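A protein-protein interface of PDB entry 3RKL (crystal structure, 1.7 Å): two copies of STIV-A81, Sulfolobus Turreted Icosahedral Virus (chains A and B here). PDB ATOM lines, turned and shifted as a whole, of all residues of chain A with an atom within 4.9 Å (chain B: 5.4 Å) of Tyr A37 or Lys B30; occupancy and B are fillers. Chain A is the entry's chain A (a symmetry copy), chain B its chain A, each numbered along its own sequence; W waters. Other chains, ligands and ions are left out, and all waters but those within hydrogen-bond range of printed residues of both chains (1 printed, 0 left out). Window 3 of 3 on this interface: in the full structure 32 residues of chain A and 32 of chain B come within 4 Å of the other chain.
The backbone carbonyl oxygen (O) of Ala A40 sits at hydrogen-bond distance from the side-chain amide nitrogen (NE2) of Gln B26.
NZ of Lys B30 lies within salt-bridge range of OE1 of Glu A44 (2.8 Å).
OE2 of Glu B27 is in salt-bridge range of NZ of Lys B30 (2.9 Å).
The side-chain carboxylate of Glu A44 lies within salt-bridge range of the side-chain amino group of Lys A41 (3.8 Å).
Ala A33 touches Ala B33.
Lys B30 touches Tyr A37 (O to CD1, 3.6 Å).
N of Tyr A37 touches CB of Ala B33 (3.8 Å).
Ile B29 touches Ala A40.
Lys B30 touches Lys A41 (NZ to NZ, 3.97 Å).
Glu A44 touches Gln B26.
Printed residues of chain B within 4 Å of Tyr A37: Lys B30 (3.6 Å) and Ala B33 (3.8 Å).
Of the printed residues of chain A, Lys B30 touches Tyr A37, Lys A41 and Glu A44.
Of the printed residues of chain A, Ala B33 touches Ala A33 (3.8 Å) and Tyr A37 (3.8 Å).
Of the printed residues of chain B, Ala A33 touches Ala B33 (3.8 Å).
Ile B35 touches none of the printed residues of chain A.
Hydrophobic or aromatic side chains of chain A within 4 Å of the printed part of chain B: Ala A33, Tyr A37 and Ala A40.
Among the printed residues, 8 pairs touch across the chains.
Among the printed residues, Asp or Glu carboxylates within 4 Å of a Lys or Arg side-chain nitrogen of the other chain: Glu A44 with Lys B30 (2.8 Å).
Ala A33 touches its own counterpart, Ala B33.
Positions printed for both chains: 33, 34 and 35.
Of the 8 pairs that touch across the chains among the printed residues, 1 has its exchanged pair printed and touching as well.
Water W1 lies within hydrogen-bond range of the side-chain amino group of Lys B30 and the side-chain amino group of Lys A41.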
ATOM      1  N   ALA A  33      23.801 -30.184   4.461  1.00  0.00           N
ATOM      2  CA  ALA A  33      24.322 -30.357   5.811  1.00  0.00           C
ATOM      3  C   ALA A  33      24.730 -29.014   6.421  1.00  0.00           C
ATOM      4  O   ALA A  33      24.499 -28.758   7.599  1.00  0.00           O
ATOM      5  CB  ALA A  33      25.507 -31.358   5.849  1.00  0.00           C
ATOM      6  N   GLU A  34      25.367 -28.187   5.609  1.00  0.00           N
ATOM      7  CA  GLU A  34      25.786 -26.861   6.029  1.00  0.00           C
ATOM      8  C   GLU A  34      24.579 -25.991   6.393  1.00  0.00           C
ATOM      9  O   GLU A  34      24.604 -25.275   7.394  1.00  0.00           O
ATOM     10  CB  GLU A  34      26.608 -26.227   4.911  1.00  0.00           C
ATOM     11  CG  GLU A  34      27.258 -24.932   5.265  1.00  0.00           C
ATOM     12  CD  GLU A  34      28.153 -24.428   4.158  1.00  0.00           C
ATOM     13  OE1 GLU A  34      27.808 -24.617   2.968  1.00  0.00           O
ATOM     14  OE2 GLU A  34      29.204 -23.841   4.479  1.00  0.00           O
ATOM     15  N   ILE A  35      23.522 -26.056   5.573  1.00  0.00           N
ATOM     16  CA  ILE A  35      22.297 -25.301   5.844  1.00  0.00           C
ATOM     17  C   ILE A  35      21.671 -25.737   7.168  1.00  0.00           C
ATOM     18  O   ILE A  35      21.266 -24.908   7.984  1.00  0.00           O
ATOM     19  CB  ILE A  35      21.297 -25.408   4.657  1.00  0.00           C
ATOM     20  CG1 ILE A  35      21.798 -24.568   3.487  1.00  0.00           C
ATOM     21  CG2 ILE A  35      19.880 -24.991   5.084  1.00  0.00           C
ATOM     22  CD1 ILE A  35      21.200 -24.950   2.142  1.00  0.00           C
ATOM     23  N   VAL A  36      21.578 -27.047   7.391  1.00  0.00           N
ATOM     24  CA  VAL A  36      21.022 -27.569   8.627  1.00  0.00           C
ATOM     25  C   VAL A  36      21.853 -27.104   9.824  1.00  0.00           C
ATOM     26  O   VAL A  36      21.303 -26.646  10.824  1.00  0.00           O
ATOM     27  CB  VAL A  36      20.912 -29.112   8.568  1.00  0.00           C
ATOM     28  CG1 VAL A  36      20.561 -29.710   9.916  1.00  0.00           C
ATOM     29  CG2 VAL A  36      19.858 -29.520   7.505  1.00  0.00           C
ATOM     30  N   TYR A  37      23.177 -27.206   9.724  1.00  0.00           N
ATOM     31  CA  TYR A  37      24.058 -26.751  10.795  1.00  0.00           C
ATOM     32  C   TYR A  37      23.834 -25.254  11.080  1.00  0.00           C
ATOM     33  O   TYR A  37      23.702 -24.833  12.238  1.00  0.00           O
ATOM     34  CB  TYR A  37      25.525 -26.990  10.435  1.00  0.00           C
ATOM     35  CG  TYR A  37      26.454 -26.509  11.511  1.00  0.00           C
ATOM     36  CD1 TYR A  37      26.792 -27.331  12.577  1.00  0.00           C
ATOM     37  CD2 TYR A  37      26.953 -25.218  11.499  1.00  0.00           C
ATOM     38  CE1 TYR A  37      27.624 -26.881  13.582  1.00  0.00           C
ATOM     39  CE2 TYR A  37      27.793 -24.762  12.509  1.00  0.00           C
ATOM     40  CZ  TYR A  37      28.119 -25.608  13.543  1.00  0.00           C
ATOM     41  OH  TYR A  37      28.948 -25.172  14.551  1.00  0.00           O
ATOM     42  N   GLN A  38      23.822 -24.462  10.018  1.00  0.00           N
ATOM     43  CA  GLN A  38      23.651 -23.011  10.155  1.00  0.00           C
ATOM     44  C   GLN A  38      22.301 -22.641  10.775  1.00  0.00           C
ATOM     45  O   GLN A  38      22.227 -21.729  11.611  1.00  0.00           O
ATOM     46  CB  GLN A  38      23.846 -22.324   8.805  1.00  0.00           C
ATOM     47  CG  GLN A  38      25.304 -22.293   8.388  1.00  0.00           C
ATOM     48  CD  GLN A  38      25.596 -21.474   7.147  1.00  0.00           C
ATOM     49  OE1 GLN A  38      24.950 -20.452   6.868  1.00  0.00           O
ATOM     50  NE2 GLN A  38      26.631 -21.892   6.419  1.00  0.00           N
ATOM     51  N   LEU A  39      21.236 -23.338  10.381  1.00  0.00           N
ATOM     52  CA  LEU A  39      19.913 -23.096  10.969  1.00  0.00           C
ATOM     53  C   LEU A  39      19.911 -23.416  12.457  1.00  0.00           C
ATOM     54  O   LEU A  39      19.414 -22.640  13.286  1.00  0.00           O
ATOM     55  CB  LEU A  39      18.812 -23.900  10.247  1.00  0.00           C
ATOM     56  CG  LEU A  39      18.264 -23.204   9.000  1.00  0.00           C
ATOM     57  CD1 LEU A  39      17.650 -24.209   8.025  1.00  0.00           C
ATOM     58  CD2 LEU A  39      17.242 -22.145   9.398  1.00  0.00           C
ATOM     59  N   ALA A  40      20.498 -24.553  12.809  1.00  0.00           N
ATOM     60  CA  ALA A  40      20.551 -24.953  14.194  1.00  0.00           C
ATOM     61  C   ALA A  40      21.340 -23.949  15.032  1.00  0.00           C
ATOM     62  O   ALA A  40      20.933 -23.605  16.146  1.00  0.00           O
ATOM     63  CB  ALA A  40      21.158 -26.357  14.321  1.00  0.00           C
ATOM     64  N   LYS A  41      22.462 -23.472  14.508  1.00  0.00           N
ATOM     65  CA  LYS A  41      23.281 -22.514  15.231  1.00  0.00           C
ATOM     66  C   LYS A  41      22.593 -21.164  15.362  1.00  0.00           C
ATOM     67  O   LYS A  41      22.753 -20.487  16.375  1.00  0.00           O
ATOM     68  CB  LYS A  41      24.632 -22.309  14.541  1.00  0.00           C
ATOM     69  CG  LYS A  41      25.599 -21.490  15.382  1.00  0.00           C
ATOM     70  CD  LYS A  41      27.065 -21.817  15.061  1.00  0.00           C
ATOM     71  CE  LYS A  41      27.950 -21.723  16.293  1.00  0.00           C
ATOM     72  NZ  LYS A  41      27.633 -22.775  17.303  1.00  0.00           N
ATOM     73  N   GLU A  44      20.033 -21.369  18.084  1.00  0.00           N
ATOM     74  CA  GLU A  44      20.736 -21.316  19.357  1.00  0.00           C
ATOM     75  C   GLU A  44      21.068 -19.882  19.766  1.00  0.00           C
ATOM     76  O   GLU A  44      20.859 -19.477  20.910  1.00  0.00           O
ATOM     77  CB  GLU A  44      22.027 -22.127  19.278  1.00  0.00           C
ATOM     78  CG  GLU A  44      22.753 -22.213  20.607  1.00  0.00           C
ATOM     79  CD  GLU A  44      24.124 -22.857  20.515  1.00  0.00           C
ATOM     80  OE1 GLU A  44      24.553 -23.267  19.420  1.00  0.00           O
ATOM     81  OE2 GLU A  44      24.790 -22.923  21.562  1.00  0.00           O
ATOM     82  N   LEU B  25      18.872 -32.139  22.186  1.00  0.00           N
ATOM     83  CA  LEU B  25      18.520 -31.940  20.774  1.00  0.00           C
ATOM     84  C   LEU B  25      19.308 -30.811  20.113  1.00  0.00           C
ATOM     85  O   LEU B  25      19.845 -30.995  19.020  1.00  0.00           O
ATOM     86  CB  LEU B  25      17.017 -31.742  20.573  1.00  0.00           C
ATOM     87  CG  LEU B  25      16.130 -32.956  20.854  1.00  0.00           C
ATOM     88  CD1 LEU B  25      14.652 -32.627  20.656  1.00  0.00           C
ATOM     89  CD2 LEU B  25      16.547 -34.138  19.967  1.00  0.00           C
ATOM     90  N   GLN B  26      19.396 -29.660  20.779  1.00  0.00           N
ATOM     91  CA  GLN B  26      20.103 -28.508  20.211  1.00  0.00           C
ATOM     92  C   GLN B  26      21.545 -28.883  19.847  1.00  0.00           C
ATOM     93  O   GLN B  26      22.025 -28.560  18.754  1.00  0.00           O
ATOM     94  CB  GLN B  26      20.070 -27.312  21.178  1.00  0.00           C
ATOM     95  CG  GLN B  26      20.915 -26.098  20.740  1.00  0.00           C
ATOM     96  CD  GLN B  26      20.341 -25.382  19.533  1.00  0.00           C
ATOM     97  OE1 GLN B  26      19.474 -24.508  19.663  1.00  0.00           O
ATOM     98  NE2 GLN B  26      20.840 -25.730  18.348  1.00  0.00           N
ATOM     99  N   GLU B  27      22.224 -29.578  20.753  1.00  0.00           N
ATOM    100  CA  GLU B  27      23.619 -29.961  20.555  1.00  0.00           C
ATOM    101  C   GLU B  27      23.749 -31.118  19.580  1.00  0.00           C
ATOM    102  O   GLU B  27      24.623 -31.114  18.705  1.00  0.00           O
ATOM    103  CB  GLU B  27      24.283 -30.324  21.893  1.00  0.00           C
ATOM    104  CG  GLU B  27      24.537 -29.123  22.779  1.00  0.00           C
ATOM    105  CD  GLU B  27      25.342 -28.047  22.075  1.00  0.00           C
ATOM    106  OE1 GLU B  27      26.485 -28.343  21.668  1.00  0.00           O
ATOM    107  OE2 GLU B  27      24.825 -26.918  21.922  1.00  0.00           O
ATOM    108  N   ASP B  28      22.871 -32.105  19.728  1.00  0.00           N
ATOM    109  CA  ASP B  28      22.872 -33.283  18.856  1.00  0.00           C
ATOM    110  C   ASP B  28      22.621 -32.913  17.395  1.00  0.00           C
ATOM    111  O   ASP B  28      23.228 -33.478  16.480  1.00  0.00           O
ATOM    112  CB  ASP B  28      21.807 -34.293  19.314  1.00  0.00           C
ATOM    113  CG  ASP B  28      22.156 -34.982  20.633  1.00  0.00           C
ATOM    114  OD1 ASP B  28      23.354 -35.123  20.980  1.00  0.00           O
ATOM    115  OD2 ASP B  28      21.209 -35.390  21.326  1.00  0.00           O
ATOM    116  N   ILE B  29      21.724 -31.958  17.160  1.00  0.00           N
ATOM    117  CA  ILE B  29      21.456 -31.532  15.789  1.00  0.00           C
ATOM    118  C   ILE B  29      22.717 -30.917  15.163  1.00  0.00           C
ATOM    119  O   ILE B  29      23.082 -31.265  14.041  1.00  0.00           O
ATOM    120  CB  ILE B  29      20.235 -30.579  15.722  1.00  0.00           C
ATOM    121  CG1 ILE B  29      18.953 -31.375  15.997  1.00  0.00           C
ATOM    122  CG2 ILE B  29      20.162 -29.897  14.368  1.00  0.00           C
ATOM    123  CD1 ILE B  29      17.733 -30.511  16.324  1.00  0.00           C
ATOM    124  N   LYS B  30      23.398 -30.023  15.885  1.00  0.00           N
ATOM    125  CA  LYS B  30      24.646 -29.436  15.374  1.00  0.00           C
ATOM    126  C   LYS B  30      25.681 -30.526  15.105  1.00  0.00           C
ATOM    127  O   LYS B  30      26.306 -30.566  14.038  1.00  0.00           O
ATOM    128  CB  LYS B  30      25.227 -28.421  16.366  1.00  0.00           C
ATOM    129  CG  LYS B  30      24.412 -27.145  16.522  1.00  0.00           C
ATOM    130  CD  LYS B  30      25.119 -26.115  17.408  1.00  0.00           C
ATOM    131  CE  LYS B  30      25.418 -26.611  18.815  1.00  0.00           C
ATOM    132  NZ  LYS B  30      26.088 -25.560  19.679  1.00  0.00           N
ATOM    133  N   ASN B  31      25.851 -31.416  16.078  1.00  0.00           N
ATOM    134  CA  ASN B  31      26.864 -32.474  15.970  1.00  0.00           C
ATOM    135  C   ASN B  31      26.593 -33.433  14.810  1.00  0.00           C
ATOM    136  O   ASN B  31      27.511 -33.808  14.064  1.00  0.00           O
ATOM    137  CB  ASN B  31      26.959 -33.261  17.265  1.00  0.00           C
ATOM    138  CG  ASN B  31      27.539 -32.457  18.412  1.00  0.00           C
ATOM    139  OD1 ASN B  31      28.173 -31.419  18.205  1.00  0.00           O
ATOM    140  ND2 ASN B  31      27.328 -32.940  19.646  1.00  0.00           N
ATOM    141  N   LEU B  32      25.335 -33.825  14.661  1.00  0.00           N
ATOM    142  CA  LEU B  32      24.955 -34.735  13.585  1.00  0.00           C
ATOM    143  C   LEU B  32      25.124 -34.066  12.210  1.00  0.00           C
ATOM    144  O   LEU B  32      25.565 -34.707  11.261  1.00  0.00           O
ATOM    145  CB  LEU B  32      23.524 -35.231  13.764  1.00  0.00           C
ATOM    146  CG  LEU B  32      23.280 -36.205  14.923  1.00  0.00           C
ATOM    147  CD1 LEU B  32      21.788 -36.346  15.201  1.00  0.00           C
ATOM    148  CD2 LEU B  32      23.886 -37.545  14.647  1.00  0.00           C
ATOM    149  N   ALA B  33      24.802 -32.775  12.096  1.00  0.00           N
ATOM    150  CA  ALA B  33      24.993 -32.077  10.829  1.00  0.00           C
ATOM    151  C   ALA B  33      26.473 -32.030  10.444  1.00  0.00           C
ATOM    152  O   ALA B  33      26.829 -32.193   9.281  1.00  0.00           O
ATOM    153  CB  ALA B  33      24.390 -30.648  10.860  1.00  0.00           C
ATOM    154  N   GLU B  34      27.313 -31.770  11.431  1.00  0.00           N
ATOM    155  CA  GLU B  34      28.752 -31.728  11.232  1.00  0.00           C
ATOM    156  C   GLU B  34      29.286 -33.094  10.788  1.00  0.00           C
ATOM    157  O   GLU B  34      30.123 -33.174   9.889  1.00  0.00           O
ATOM    158  CB  GLU B  34      29.415 -31.269  12.526  1.00  0.00           C
ATOM    159  CG  GLU B  34      30.880 -31.007  12.423  1.00  0.00           C
ATOM    160  CD  GLU B  34      31.443 -30.437  13.704  1.00  0.00           C
ATOM    161  OE1 GLU B  34      30.985 -30.840  14.798  1.00  0.00           O
ATOM    162  OE2 GLU B  34      32.347 -29.585  13.615  1.00  0.00           O
ATOM    163  N   ILE B  35      28.797 -34.166  11.425  1.00  0.00           N
ATOM    164  CA  ILE B  35      29.204 -35.524  11.056  1.00  0.00           C
ATOM    165  C   ILE B  35      28.815 -35.835   9.612  1.00  0.00           C
ATOM    166  O   ILE B  35      29.609 -36.378   8.841  1.00  0.00           O
ATOM    167  CB  ILE B  35      28.637 -36.571  12.057  1.00  0.00           C
ATOM    168  CG1 ILE B  35      29.395 -36.483  13.377  1.00  0.00           C
ATOM    169  CG2 ILE B  35      28.692 -37.990  11.469  1.00  0.00           C
ATOM    170  CD1 ILE B  35      28.658 -37.085  14.563  1.00  0.00           C
HETATM  171  O   HOH W   1      28.707 -25.190  18.939  1.00  0.00           O
